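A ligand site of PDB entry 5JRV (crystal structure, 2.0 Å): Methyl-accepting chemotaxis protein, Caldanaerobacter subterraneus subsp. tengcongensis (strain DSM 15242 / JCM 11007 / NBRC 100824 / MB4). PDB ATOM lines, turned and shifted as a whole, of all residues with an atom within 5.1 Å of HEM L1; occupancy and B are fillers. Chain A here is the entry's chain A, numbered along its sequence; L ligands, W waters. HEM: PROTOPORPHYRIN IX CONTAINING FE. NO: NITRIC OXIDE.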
ATOM      1  N   MET A   1       5.036  21.576 -12.892  1.00  0.00           N
ATOM      2  CA  MET A   1       5.423  21.493 -11.490  1.00  0.00           C
ATOM      3  C   MET A   1       6.808  22.100 -11.285  1.00  0.00           C
ATOM      4  O   MET A   1       7.724  21.833 -12.070  1.00  0.00           O
ATOM      5  CB  MET A   1       5.415  20.038 -11.026  1.00  0.00           C
ATOM      6  CG  MET A   1       5.196  19.882  -9.530  1.00  0.00           C
ATOM      7  SD  MET A   1       3.480  20.218  -9.118  1.00  0.00           S
ATOM      8  CE  MET A   1       2.678  18.888 -10.002  1.00  0.00           C
ATOM      9  N   LYS A   2       6.946  22.932 -10.253  1.00  0.00           N
ATOM     10  CA  LYS A   2       8.245  23.523  -9.924  1.00  0.00           C
ATOM     11  C   LYS A   2       9.289  22.418  -9.781  1.00  0.00           C
ATOM     12  O   LYS A   2       9.053  21.420  -9.107  1.00  0.00           O
ATOM     13  CB  LYS A   2       8.136  24.352  -8.644  1.00  0.00           C
ATOM     14  CG  LYS A   2       9.473  24.761  -8.011  1.00  0.00           C
ATOM     15  CD  LYS A   2       9.359  25.931  -6.984  1.00  0.00           C
ATOM     16  CE  LYS A   2      10.497  25.845  -5.922  1.00  0.00           C
ATOM     17  NZ  LYS A   2      10.327  26.396  -4.515  1.00  0.00           N
ATOM     18  N   ILE A   5      10.376  21.031  -6.348  1.00  0.00           N
ATOM     19  CA  ILE A   5       9.429  20.161  -5.673  1.00  0.00           C
ATOM     20  C   ILE A   5       9.496  18.745  -6.244  1.00  0.00           C
ATOM     21  O   ILE A   5       9.411  17.758  -5.504  1.00  0.00           O
ATOM     22  CB  ILE A   5       8.010  20.742  -5.772  1.00  0.00           C
ATOM     23  CG1 ILE A   5       8.017  22.183  -5.266  1.00  0.00           C
ATOM     24  CG2 ILE A   5       7.017  19.899  -4.978  1.00  0.00           C
ATOM     25  CD1 ILE A   5       8.491  22.352  -3.837  1.00  0.00           C
ATOM     26  N   TRP A   9      10.328  15.124  -4.361  1.00  0.00           N
ATOM     27  CA  TRP A   9       9.613  13.871  -4.561  1.00  0.00           C
ATOM     28  C   TRP A   9      10.569  12.735  -4.916  1.00  0.00           C
ATOM     29  O   TRP A   9      10.387  11.602  -4.458  1.00  0.00           O
ATOM     30  CB  TRP A   9       8.542  14.047  -5.646  1.00  0.00           C
ATOM     31  CG  TRP A   9       7.458  15.009  -5.257  1.00  0.00           C
ATOM     32  CD1 TRP A   9       7.156  15.430  -3.982  1.00  0.00           C
ATOM     33  CD2 TRP A   9       6.541  15.675  -6.125  1.00  0.00           C
ATOM     34  NE1 TRP A   9       6.108  16.311  -4.016  1.00  0.00           N
ATOM     35  CE2 TRP A   9       5.705  16.481  -5.318  1.00  0.00           C
ATOM     36  CE3 TRP A   9       6.335  15.660  -7.509  1.00  0.00           C
ATOM     37  CZ2 TRP A   9       4.698  17.265  -5.856  1.00  0.00           C
ATOM     38  CZ3 TRP A   9       5.328  16.446  -8.036  1.00  0.00           C
ATOM     39  CH2 TRP A   9       4.519  17.236  -7.209  1.00  0.00           C
ATOM     40  N   ILE A  75       7.162  15.848   4.040  1.00  0.00           N
ATOM     41  CA  ILE A  75       7.306  16.854   5.091  1.00  0.00           C
ATOM     42  C   ILE A  75       8.707  16.786   5.701  1.00  0.00           C
ATOM     43  O   ILE A  75       9.353  17.820   5.920  1.00  0.00           O
ATOM     44  CB  ILE A  75       6.210  16.662   6.159  1.00  0.00           C
ATOM     45  CG1 ILE A  75       4.829  16.952   5.561  1.00  0.00           C
ATOM     46  CG2 ILE A  75       6.483  17.545   7.373  1.00  0.00           C
ATOM     47  CD1 ILE A  75       4.701  18.352   4.996  1.00  0.00           C
ATOM     48  N   PHE A  78      10.986  18.271   3.154  1.00  0.00           N
ATOM     49  CA  PHE A  78      10.841  19.722   3.199  1.00  0.00           C
ATOM     50  C   PHE A  78      11.565  20.319   4.398  1.00  0.00           C
ATOM     51  O   PHE A  78      12.144  21.408   4.299  1.00  0.00           O
ATOM     52  CB  PHE A  78       9.356  20.102   3.267  1.00  0.00           C
ATOM     53  CG  PHE A  78       8.642  20.063   1.948  1.00  0.00           C
ATOM     54  CD1 PHE A  78       9.321  20.282   0.756  1.00  0.00           C
ATOM     55  CD2 PHE A  78       7.271  19.855   1.906  1.00  0.00           C
ATOM     56  CE1 PHE A  78       8.631  20.260  -0.455  1.00  0.00           C
ATOM     57  CE2 PHE A  78       6.589  19.842   0.714  1.00  0.00           C
ATOM     58  CZ  PHE A  78       7.258  20.042  -0.476  1.00  0.00           C
ATOM     59  N   PHE A  82      13.866  23.177   3.292  1.00  0.00           N
ATOM     60  CA  PHE A  82      13.307  24.485   3.626  1.00  0.00           C
ATOM     61  C   PHE A  82      13.211  24.646   5.140  1.00  0.00           C
ATOM     62  O   PHE A  82      12.115  24.845   5.676  1.00  0.00           O
ATOM     63  CB  PHE A  82      11.920  24.664   3.001  1.00  0.00           C
ATOM     64  CG  PHE A  82      11.873  24.495   1.512  1.00  0.00           C
ATOM     65  CD1 PHE A  82      12.294  25.506   0.660  1.00  0.00           C
ATOM     66  CD2 PHE A  82      11.364  23.329   0.953  1.00  0.00           C
ATOM     67  CE1 PHE A  82      12.233  25.339  -0.709  1.00  0.00           C
ATOM     68  CE2 PHE A  82      11.311  23.167  -0.427  1.00  0.00           C
ATOM     69  CZ  PHE A  82      11.747  24.179  -1.258  1.00  0.00           C
ATOM     70  N   TYR A  85      11.063  27.360   7.071  1.00  0.00           N
ATOM     71  CA  TYR A  85       9.606  27.277   7.025  1.00  0.00           C
ATOM     72  C   TYR A  85       9.037  26.489   8.195  1.00  0.00           C
ATOM     73  O   TYR A  85       7.838  26.565   8.456  1.00  0.00           O
ATOM     74  CB  TYR A  85       9.157  26.654   5.712  1.00  0.00           C
ATOM     75  CG  TYR A  85       9.215  27.628   4.571  1.00  0.00           C
ATOM     76  CD1 TYR A  85      10.425  28.186   4.171  1.00  0.00           C
ATOM     77  CD2 TYR A  85       8.066  28.017   3.895  1.00  0.00           C
ATOM     78  CE1 TYR A  85      10.483  29.096   3.139  1.00  0.00           C
ATOM     79  CE2 TYR A  85       8.116  28.921   2.864  1.00  0.00           C
ATOM     80  CZ  TYR A  85       9.332  29.459   2.486  1.00  0.00           C
ATOM     81  OH  TYR A  85       9.396  30.361   1.455  1.00  0.00           O
ATOM     82  N   PHE A  86       9.880  25.747   8.912  1.00  0.00           N
ATOM     83  CA  PHE A  86       9.456  24.930  10.042  1.00  0.00           C
ATOM     84  C   PHE A  86       9.890  25.480  11.385  1.00  0.00           C
ATOM     85  O   PHE A  86       9.092  25.473  12.332  1.00  0.00           O
ATOM     86  CB  PHE A  86       9.995  23.508   9.864  1.00  0.00           C
ATOM     87  CG  PHE A  86       9.413  22.781   8.688  1.00  0.00           C
ATOM     88  CD1 PHE A  86       9.897  22.991   7.410  1.00  0.00           C
ATOM     89  CD2 PHE A  86       8.365  21.880   8.855  1.00  0.00           C
ATOM     90  CE1 PHE A  86       9.360  22.335   6.315  1.00  0.00           C
ATOM     91  CE2 PHE A  86       7.814  21.226   7.770  1.00  0.00           C
ATOM     92  CZ  PHE A  86       8.315  21.450   6.501  1.00  0.00           C
ATOM     93  N   PHE A  94       2.002  26.817  10.477  1.00  0.00           N
ATOM     94  CA  PHE A  94       2.551  26.203   9.271  1.00  0.00           C
ATOM     95  C   PHE A  94       1.465  25.950   8.239  1.00  0.00           C
ATOM     96  O   PHE A  94       1.582  26.355   7.077  1.00  0.00           O
ATOM     97  CB  PHE A  94       3.253  24.907   9.677  1.00  0.00           C
ATOM     98  CG  PHE A  94       3.790  24.123   8.533  1.00  0.00           C
ATOM     99  CD1 PHE A  94       4.994  24.466   7.958  1.00  0.00           C
ATOM    100  CD2 PHE A  94       3.104  23.018   8.062  1.00  0.00           C
ATOM    101  CE1 PHE A  94       5.502  23.733   6.908  1.00  0.00           C
ATOM    102  CE2 PHE A  94       3.604  22.279   7.013  1.00  0.00           C
ATOM    103  CZ  PHE A  94       4.810  22.636   6.436  1.00  0.00           C
ATOM    104  N   LEU A  95       0.371  25.294   8.659  1.00  0.00           N
ATOM    105  CA  LEU A  95      -0.730  25.029   7.740  1.00  0.00           C
ATOM    106  C   LEU A  95      -1.328  26.316   7.191  1.00  0.00           C
ATOM    107  O   LEU A  95      -1.663  26.398   5.999  1.00  0.00           O
ATOM    108  CB  LEU A  95      -1.799  24.207   8.453  1.00  0.00           C
ATOM    109  CG  LEU A  95      -1.357  22.775   8.782  1.00  0.00           C
ATOM    110  CD1 LEU A  95      -2.421  22.043   9.594  1.00  0.00           C
ATOM    111  CD2 LEU A  95      -1.045  22.028   7.497  1.00  0.00           C
ATOM    112  N   MET A  98       0.417  28.176   4.217  1.00  0.00           N
ATOM    113  CA  MET A  98       0.728  27.411   3.014  1.00  0.00           C
ATOM    114  C   MET A  98       0.145  28.046   1.760  1.00  0.00           C
ATOM    115  O   MET A  98       0.794  28.065   0.714  1.00  0.00           O
ATOM    116  CB  MET A  98       0.241  25.967   3.165  1.00  0.00           C
ATOM    117  CG  MET A  98       1.141  25.095   4.039  1.00  0.00           C
ATOM    118  SD  MET A  98       2.818  24.998   3.387  1.00  0.00           S
ATOM    119  CE  MET A  98       3.711  26.055   4.524  1.00  0.00           C
ATOM    120  N   VAL A 101       2.359  30.818   0.747  1.00  0.00           N
ATOM    121  CA  VAL A 101       3.632  30.244   0.305  1.00  0.00           C
ATOM    122  C   VAL A 101       3.524  29.750  -1.133  1.00  0.00           C
ATOM    123  O   VAL A 101       4.404  30.015  -1.953  1.00  0.00           O
ATOM    124  CB  VAL A 101       4.066  29.115   1.262  1.00  0.00           C
ATOM    125  CG1 VAL A 101       5.052  28.186   0.588  1.00  0.00           C
ATOM    126  CG2 VAL A 101       4.662  29.708   2.535  1.00  0.00           C
ATOM    127  N   HIS A 102       2.444  29.028  -1.451  1.00  0.00           N
ATOM    128  CA  HIS A 102       2.321  28.456  -2.788  1.00  0.00           C
ATOM    129  C   HIS A 102       2.057  29.532  -3.833  1.00  0.00           C
ATOM    130  O   HIS A 102       2.532  29.416  -4.969  1.00  0.00           O
ATOM    131  CB  HIS A 102       1.236  27.378  -2.800  1.00  0.00           C
ATOM    132  CG  HIS A 102       1.658  26.106  -2.137  1.00  0.00           C
ATOM    133  ND1 HIS A 102       1.828  26.001  -0.767  1.00  0.00           N
ATOM    134  CD2 HIS A 102       1.956  24.892  -2.648  1.00  0.00           C
ATOM    135  CE1 HIS A 102       2.224  24.771  -0.472  1.00  0.00           C
ATOM    136  NE2 HIS A 102       2.287  24.075  -1.597  1.00  0.00           N
ATOM    137  N   LEU A 105       5.772  31.292  -3.999  1.00  0.00           N
ATOM    138  CA  LEU A 105       6.817  30.423  -4.540  1.00  0.00           C
ATOM    139  C   LEU A 105       6.609  30.102  -6.017  1.00  0.00           C
ATOM    140  O   LEU A 105       7.503  29.529  -6.632  1.00  0.00           O
ATOM    141  CB  LEU A 105       6.898  29.097  -3.772  1.00  0.00           C
ATOM    142  CG  LEU A 105       7.554  29.121  -2.400  1.00  0.00           C
ATOM    143  CD1 LEU A 105       7.792  27.693  -1.955  1.00  0.00           C
ATOM    144  CD2 LEU A 105       8.852  29.904  -2.417  1.00  0.00           C
ATOM    145  N   THR A 106       5.448  30.442  -6.577  1.00  0.00           N
ATOM    146  CA  THR A 106       5.155  30.240  -7.986  1.00  0.00           C
ATOM    147  C   THR A 106       4.832  31.562  -8.677  1.00  0.00           C
ATOM    148  O   THR A 106       4.602  31.571  -9.893  1.00  0.00           O
ATOM    149  CB  THR A 106       3.975  29.264  -8.139  1.00  0.00           C
ATOM    150  OG1 THR A 106       4.033  28.600  -9.408  1.00  0.00           O
ATOM    151  CG2 THR A 106       2.671  30.021  -8.041  1.00  0.00           C
ATOM    152  N   THR A 113       0.187  27.765 -11.855  1.00  0.00           N
ATOM    153  CA  THR A 113      -1.035  27.116 -11.392  1.00  0.00           C
ATOM    154  C   THR A 113      -0.784  26.445 -10.054  1.00  0.00           C
ATOM    155  O   THR A 113      -0.817  25.214  -9.941  1.00  0.00           O
ATOM    156  CB  THR A 113      -1.537  26.098 -12.413  1.00  0.00           C
ATOM    157  OG1 THR A 113      -0.491  25.165 -12.724  1.00  0.00           O
ATOM    158  CG2 THR A 113      -2.014  26.774 -13.695  1.00  0.00           C
ATOM    159  N   PRO A 114      -0.552  27.226  -8.998  1.00  0.00           N
ATOM    160  CA  PRO A 114      -0.343  26.620  -7.698  1.00  0.00           C
ATOM    161  C   PRO A 114      -1.661  26.108  -7.149  1.00  0.00           C
ATOM    162  O   PRO A 114      -2.735  26.615  -7.509  1.00  0.00           O
ATOM    163  CB  PRO A 114       0.175  27.788  -6.837  1.00  0.00           C
ATOM    164  CG  PRO A 114      -0.529  28.961  -7.420  1.00  0.00           C
ATOM    165  CD  PRO A 114      -0.594  28.700  -8.908  1.00  0.00           C
ATOM    166  N   PRO A 115      -1.634  25.094  -6.298  1.00  0.00           N
ATOM    167  CA  PRO A 115      -2.843  24.753  -5.541  1.00  0.00           C
ATOM    168  C   PRO A 115      -3.195  25.904  -4.618  1.00  0.00           C
ATOM    169  O   PRO A 115      -2.321  26.554  -4.044  1.00  0.00           O
ATOM    170  CB  PRO A 115      -2.439  23.506  -4.751  1.00  0.00           C
ATOM    171  CG  PRO A 115      -0.943  23.615  -4.638  1.00  0.00           C
ATOM    172  CD  PRO A 115      -0.485  24.252  -5.908  1.00  0.00           C
ATOM    173  N   LEU A 117      -4.849  26.698  -1.059  1.00  0.00           N
ATOM    174  CA  LEU A 117      -4.809  25.940   0.183  1.00  0.00           C
ATOM    175  C   LEU A 117      -5.375  26.777   1.322  1.00  0.00           C
ATOM    176  O   LEU A 117      -4.872  26.731   2.445  1.00  0.00           O
ATOM    177  CB  LEU A 117      -3.385  25.502   0.507  1.00  0.00           C
ATOM    178  CG  LEU A 117      -2.699  24.592  -0.525  1.00  0.00           C
ATOM    179  CD1 LEU A 117      -1.219  24.501  -0.246  1.00  0.00           C
ATOM    180  CD2 LEU A 117      -3.329  23.201  -0.488  1.00  0.00           C
ATOM    181  N   MET A 129      -9.715  23.779   5.830  1.00  0.00           N
ATOM    182  CA  MET A 129      -8.709  23.929   4.800  1.00  0.00           C
ATOM    183  C   MET A 129      -9.258  23.309   3.529  1.00  0.00           C
ATOM    184  O   MET A 129      -9.744  22.171   3.551  1.00  0.00           O
ATOM    185  CB  MET A 129      -7.389  23.264   5.214  1.00  0.00           C
ATOM    186  CG  MET A 129      -6.213  23.577   4.321  1.00  0.00           C
ATOM    187  SD  MET A 129      -4.661  23.216   5.146  1.00  0.00           S
ATOM    188  CE  MET A 129      -3.487  23.881   3.967  1.00  0.00           C
ATOM    189  N   TYR A 131      -8.274  22.347  -0.336  1.00  0.00           N
ATOM    190  CA  TYR A 131      -7.432  22.149  -1.500  1.00  0.00           C
ATOM    191  C   TYR A 131      -8.248  22.445  -2.758  1.00  0.00           C
ATOM    192  O   TYR A 131      -9.354  21.910  -2.927  1.00  0.00           O
ATOM    193  CB  TYR A 131      -6.922  20.708  -1.514  1.00  0.00           C
ATOM    194  CG  TYR A 131      -6.312  20.248  -2.802  1.00  0.00           C
ATOM    195  CD1 TYR A 131      -5.023  20.631  -3.152  1.00  0.00           C
ATOM    196  CD2 TYR A 131      -7.006  19.404  -3.658  1.00  0.00           C
ATOM    197  CE1 TYR A 131      -4.450  20.204  -4.332  1.00  0.00           C
ATOM    198  CE2 TYR A 131      -6.435  18.963  -4.836  1.00  0.00           C
ATOM    199  CZ  TYR A 131      -5.157  19.364  -5.168  1.00  0.00           C
ATOM    200  OH  TYR A 131      -4.577  18.944  -6.340  1.00  0.00           O
ATOM    201  N   SER A 133      -7.389  22.719  -6.955  1.00  0.00           N
ATOM    202  CA  SER A 133      -6.391  22.619  -7.994  1.00  0.00           C
ATOM    203  C   SER A 133      -6.969  21.868  -9.187  1.00  0.00           C
ATOM    204  O   SER A 133      -7.846  21.024  -9.031  1.00  0.00           O
ATOM    205  CB  SER A 133      -5.127  21.906  -7.502  1.00  0.00           C
ATOM    206  OG  SER A 133      -4.270  21.587  -8.581  1.00  0.00           O
ATOM    207  N   ARG A 135      -5.168  19.783 -10.684  1.00  0.00           N
ATOM    208  CA  ARG A 135      -4.306  18.613 -10.770  1.00  0.00           C
ATOM    209  C   ARG A 135      -4.826  17.383 -10.040  1.00  0.00           C
ATOM    210  O   ARG A 135      -4.290  16.286 -10.259  1.00  0.00           O
ATOM    211  CB  ARG A 135      -2.902  18.938 -10.229  1.00  0.00           C
ATOM    212  CG  ARG A 135      -2.146  20.006 -10.995  1.00  0.00           C
ATOM    213  CD  ARG A 135      -0.654  19.888 -10.693  1.00  0.00           C
ATOM    214  NE  ARG A 135       0.159  20.835 -11.455  1.00  0.00           N
ATOM    215  CZ  ARG A 135       0.567  22.003 -10.975  1.00  0.00           C
ATOM    216  NH1 ARG A 135       0.239  22.385  -9.744  1.00  0.00           N
ATOM    217  NH2 ARG A 135       1.299  22.809 -11.737  1.00  0.00           N
ATOM    218  N   MET A 137      -4.706  16.147  -6.895  1.00  0.00           N
ATOM    219  CA  MET A 137      -3.727  15.406  -6.100  1.00  0.00           C
ATOM    220  C   MET A 137      -4.197  15.302  -4.655  1.00  0.00           C
ATOM    221  O   MET A 137      -3.551  15.747  -3.708  1.00  0.00           O
ATOM    222  CB  MET A 137      -2.353  16.059  -6.224  1.00  0.00           C
ATOM    223  CG  MET A 137      -1.802  15.948  -7.645  1.00  0.00           C
ATOM    224  SD  MET A 137      -0.301  16.899  -7.960  1.00  0.00           S
ATOM    225  CE  MET A 137       0.883  15.953  -7.003  1.00  0.00           C
ATOM    226  N   TYR A 140      -1.911  13.227  -2.062  1.00  0.00           N
ATOM    227  CA  TYR A 140      -0.726  13.987  -1.690  1.00  0.00           C
ATOM    228  C   TYR A 140      -1.072  15.063  -0.667  1.00  0.00           C
ATOM    229  O   TYR A 140      -0.399  15.193   0.369  1.00  0.00           O
ATOM    230  CB  TYR A 140      -0.108  14.599  -2.951  1.00  0.00           C
ATOM    231  CG  TYR A 140       1.169  15.367  -2.713  1.00  0.00           C
ATOM    232  CD1 TYR A 140       2.262  14.760  -2.109  1.00  0.00           C
ATOM    233  CD2 TYR A 140       1.290  16.687  -3.113  1.00  0.00           C
ATOM    234  CE1 TYR A 140       3.438  15.458  -1.891  1.00  0.00           C
ATOM    235  CE2 TYR A 140       2.453  17.400  -2.906  1.00  0.00           C
ATOM    236  CZ  TYR A 140       3.524  16.790  -2.291  1.00  0.00           C
ATOM    237  OH  TYR A 140       4.686  17.489  -2.083  1.00  0.00           O
ATOM    238  N   PHE A 141      -2.143  15.826  -0.918  1.00  0.00           N
ATOM    239  CA  PHE A 141      -2.604  16.840   0.015  1.00  0.00           C
ATOM    240  C   PHE A 141      -2.876  16.259   1.394  1.00  0.00           C
ATOM    241  O   PHE A 141      -2.426  16.787   2.416  1.00  0.00           O
ATOM    242  CB  PHE A 141      -3.859  17.514  -0.554  1.00  0.00           C
ATOM    243  CG  PHE A 141      -4.602  18.373   0.425  1.00  0.00           C
ATOM    244  CD1 PHE A 141      -4.140  19.642   0.730  1.00  0.00           C
ATOM    245  CD2 PHE A 141      -5.782  17.934   1.002  1.00  0.00           C
ATOM    246  CE1 PHE A 141      -4.840  20.448   1.614  1.00  0.00           C
ATOM    247  CE2 PHE A 141      -6.476  18.733   1.886  1.00  0.00           C
ATOM    248  CZ  PHE A 141      -6.008  19.995   2.202  1.00  0.00           C
ATOM    249  N   LEU A 144       0.322  15.127   3.173  1.00  0.00           N
ATOM    250  CA  LEU A 144       1.110  16.252   3.679  1.00  0.00           C
ATOM    251  C   LEU A 144       0.575  16.739   5.022  1.00  0.00           C
ATOM    252  O   LEU A 144       1.342  17.132   5.903  1.00  0.00           O
ATOM    253  CB  LEU A 144       1.118  17.392   2.660  1.00  0.00           C
ATOM    254  CG  LEU A 144       1.958  17.182   1.406  1.00  0.00           C
ATOM    255  CD1 LEU A 144       1.530  18.136   0.320  1.00  0.00           C
ATOM    256  CD2 LEU A 144       3.443  17.367   1.711  1.00  0.00           C
ATOM    257  N   ILE A 145      -0.755  16.739   5.185  1.00  0.00           N
ATOM    258  CA  ILE A 145      -1.326  17.115   6.472  1.00  0.00           C
ATOM    259  C   ILE A 145      -0.954  16.102   7.547  1.00  0.00           C
ATOM    260  O   ILE A 145      -0.579  16.480   8.670  1.00  0.00           O
ATOM    261  CB  ILE A 145      -2.855  17.260   6.349  1.00  0.00           C
ATOM    262  CG1 ILE A 145      -3.202  18.407   5.388  1.00  0.00           C
ATOM    263  CG2 ILE A 145      -3.492  17.488   7.706  1.00  0.00           C
ATOM    264  CD1 ILE A 145      -4.669  18.489   5.049  1.00  0.00           C
ATOM    265  N   SER A 148       2.596  16.536   8.427  1.00  0.00           N
ATOM    266  CA  SER A 148       2.792  17.758   9.188  1.00  0.00           C
ATOM    267  C   SER A 148       2.479  17.538  10.664  1.00  0.00           C
ATOM    268  O   SER A 148       3.225  17.991  11.537  1.00  0.00           O
ATOM    269  CB  SER A 148       1.940  18.879   8.625  1.00  0.00           C
ATOM    270  OG  SER A 148       2.377  19.227   7.311  1.00  0.00           O
HETATM  271  CHA HEM L   1       2.826  21.518  -4.879  1.00  0.00           C
HETATM  272  CHB HEM L   1       5.742  24.300  -2.220  1.00  0.00           C
HETATM  273  CHC HEM L   1       3.984  22.204   1.761  1.00  0.00           C
HETATM  274  CHD HEM L   1       0.095  21.209  -0.906  1.00  0.00           C
HETATM  275  C1A HEM L   1       3.762  22.462  -4.535  1.00  0.00           C
HETATM  276  C2A HEM L   1       4.507  23.330  -5.417  1.00  0.00           C
HETATM  277  C3A HEM L   1       5.311  24.096  -4.684  1.00  0.00           C
HETATM  278  C4A HEM L   1       5.103  23.745  -3.295  1.00  0.00           C
HETATM  279  CMA HEM L   1       6.292  25.175  -5.205  1.00  0.00           C
HETATM  280  CAA HEM L   1       4.422  23.381  -6.963  1.00  0.00           C
HETATM  281  CBA HEM L   1       3.258  24.269  -7.389  1.00  0.00           C
HETATM  282  CGA HEM L   1       3.192  24.250  -8.897  1.00  0.00           C
HETATM  283  O1A HEM L   1       2.139  24.650  -9.456  1.00  0.00           O
HETATM  284  O2A HEM L   1       4.199  23.842  -9.525  1.00  0.00           O
HETATM  285  C1B HEM L   1       5.635  23.854  -0.922  1.00  0.00           C
HETATM  286  C2B HEM L   1       6.599  24.039   0.141  1.00  0.00           C
HETATM  287  C3B HEM L   1       6.126  23.461   1.242  1.00  0.00           C
HETATM  288  C4B HEM L   1       4.829  22.887   0.931  1.00  0.00           C
HETATM  289  CMB HEM L   1       7.954  24.769   0.038  1.00  0.00           C
HETATM  290  CAB HEM L   1       6.900  23.460   2.584  1.00  0.00           C
HETATM  291  CBB HEM L   1       6.461  22.819   3.673  1.00  0.00           C
HETATM  292  C1C HEM L   1       2.700  21.855   1.422  1.00  0.00           C
HETATM  293  C2C HEM L   1       1.616  21.541   2.333  1.00  0.00           C
HETATM  294  C3C HEM L   1       0.534  21.245   1.589  1.00  0.00           C
HETATM  295  C4C HEM L   1       0.904  21.404   0.200  1.00  0.00           C
HETATM  296  CMC HEM L   1       1.790  21.521   3.864  1.00  0.00           C
HETATM  297  CAC HEM L   1      -0.891  20.856   2.044  1.00  0.00           C
HETATM  298  CBC HEM L   1      -1.395  21.198   3.244  1.00  0.00           C
HETATM  299  C1D HEM L   1       0.566  21.013  -2.173  1.00  0.00           C
HETATM  300  C2D HEM L   1      -0.029  20.165  -3.192  1.00  0.00           C
HETATM  301  C3D HEM L   1       0.719  20.244  -4.298  1.00  0.00           C
HETATM  302  C4D HEM L   1       1.820  21.145  -4.023  1.00  0.00           C
HETATM  303  CMD HEM L   1      -1.298  19.317  -3.036  1.00  0.00           C
HETATM  304  CAD HEM L   1       0.430  19.480  -5.607  1.00  0.00           C
HETATM  305  CBD HEM L   1       0.146  20.452  -6.750  1.00  0.00           C
HETATM  306  CGD HEM L   1      -1.339  20.504  -7.003  1.00  0.00           C
HETATM  307  O1D HEM L   1      -1.796  21.319  -7.850  1.00  0.00           O
HETATM  308  O2D HEM L   1      -2.082  19.729  -6.345  1.00  0.00           O
HETATM  309  NA  HEM L   1       4.156  22.745  -3.239  1.00  0.00           N
HETATM  310  NB  HEM L   1       4.571  23.143  -0.405  1.00  0.00           N
HETATM  311  NC  HEM L   1       2.230  21.768   0.133  1.00  0.00           N
HETATM  312  ND  HEM L   1       1.700  21.598  -2.716  1.00  0.00           N
HETATM  313 FE   HEM L   1       3.175  22.287  -1.556  1.00  0.00          FE
HETATM  314  N    NO L   2       3.814  20.603  -1.442  1.00  0.00           N
HETATM  315  O    NO L   2       4.659  20.135  -2.523  1.00  0.00           O
HETATM  316  O   HOH W   1       2.270  26.495 -11.020  1.00  0.00           O
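Water W1 lies within hydrogen-bond range of an oxygen (O1A) of HEM L1 (2.4 Å), the backbone NH of Thr 113 (2.6 Å) and the side-chain hydroxyl of Thr 106 (3.2 Å).
O2A of HEM L1 lies close to SD of Met 1, 3.7 Å away. SD of Met 137 sits close to O2D of HEM L1 (3.7 Å). Merely in contact with HEM L1: Ile 5 (3.4 Å), Phe 78 (3.5 Å), Phe 82 (3.7 Å), Phe 86 (3.6 Å), Phe 94 (3.2 Å), Met 98 (3.4 Å), Leu 105 (3.5 Å), Pro 114 (3.6 Å), Pro 115 (3.8 Å), Leu 117 (3.6 Å), Met 129 (3.5 Å), Tyr 140 (3.6 Å), Phe 141 (3.7 Å), Leu 144 (3.3 Å) and Ile 145 (3.96 Å). Hydrophobic or aromatic side chains within 4 Å of HEM L1: Met 1, Ile 5, Phe 78, Phe 82, Phe 86, Phe 94, Met 98, His 102, Leu 105, Pro 115, Leu 117, Met 129, Tyr 131, Met 137, Tyr 140, Phe 141, Leu 144 and Ile 145. Of the 30 residues printed, 23 come within 4 Å of HEM L1.
The side-chain hydroxyl of Ser 133 is in hydrogen-bond range of the backbone NH of Arg 135, at 2.9 Å. The guanidinium group (NH1) of Arg 135 lies within hydrogen-bond range of the backbone carbonyl oxygen (O) of Thr 113, 3.0 Å away. The backbone carbonyl oxygen of Met 98 sits at hydrogen-bond distance from a ring nitrogen (ND1) of His 102, 2.7 Å away. The backbone carbonyl oxygen of Leu 144 lies within hydrogen-bond range of the side-chain hydroxyl of Ser 148. OH of Tyr 131 sits at hydrogen-bond distance from N of Met 137. OH of Tyr 140 sits at hydrogen-bond distance from NE1 of Trp 9 (2.7 Å). The side-chain hydroxyl (OG) of Ser 133 lies close to the side-chain hydroxyl (OH) of Tyr 131 (3.5 Å).
An iron atom (FE) of HEM L1 is bound by a nitrogen (N) of NO L2 (1.8 Å).
The side-chain hydroxyl (OH) of Tyr 140 lies within hydrogen-bond range of an oxygen (O) of NO L2, 2.7 Å away. NH1 of Arg 135 is in salt-bridge range of O1A of HEM L1 (3.0 Å). N of Lys 2 is in hydrogen-bond range of O2A of HEM L1 (3.0 Å). The side-chain hydroxyl (OH) of Tyr 131 lies within hydrogen-bond range of an oxygen (O2D) of HEM L1, 2.6 Å away. The side-chain hydroxyl (OG) of Ser 133 is in hydrogen-bond range of an oxygen (O1D) of HEM L1. NE2 of His 102 binds FE of HEM L1 (2.0 Å). O of Thr 113 lies close to O1A of HEM L1 (3.0 Å).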
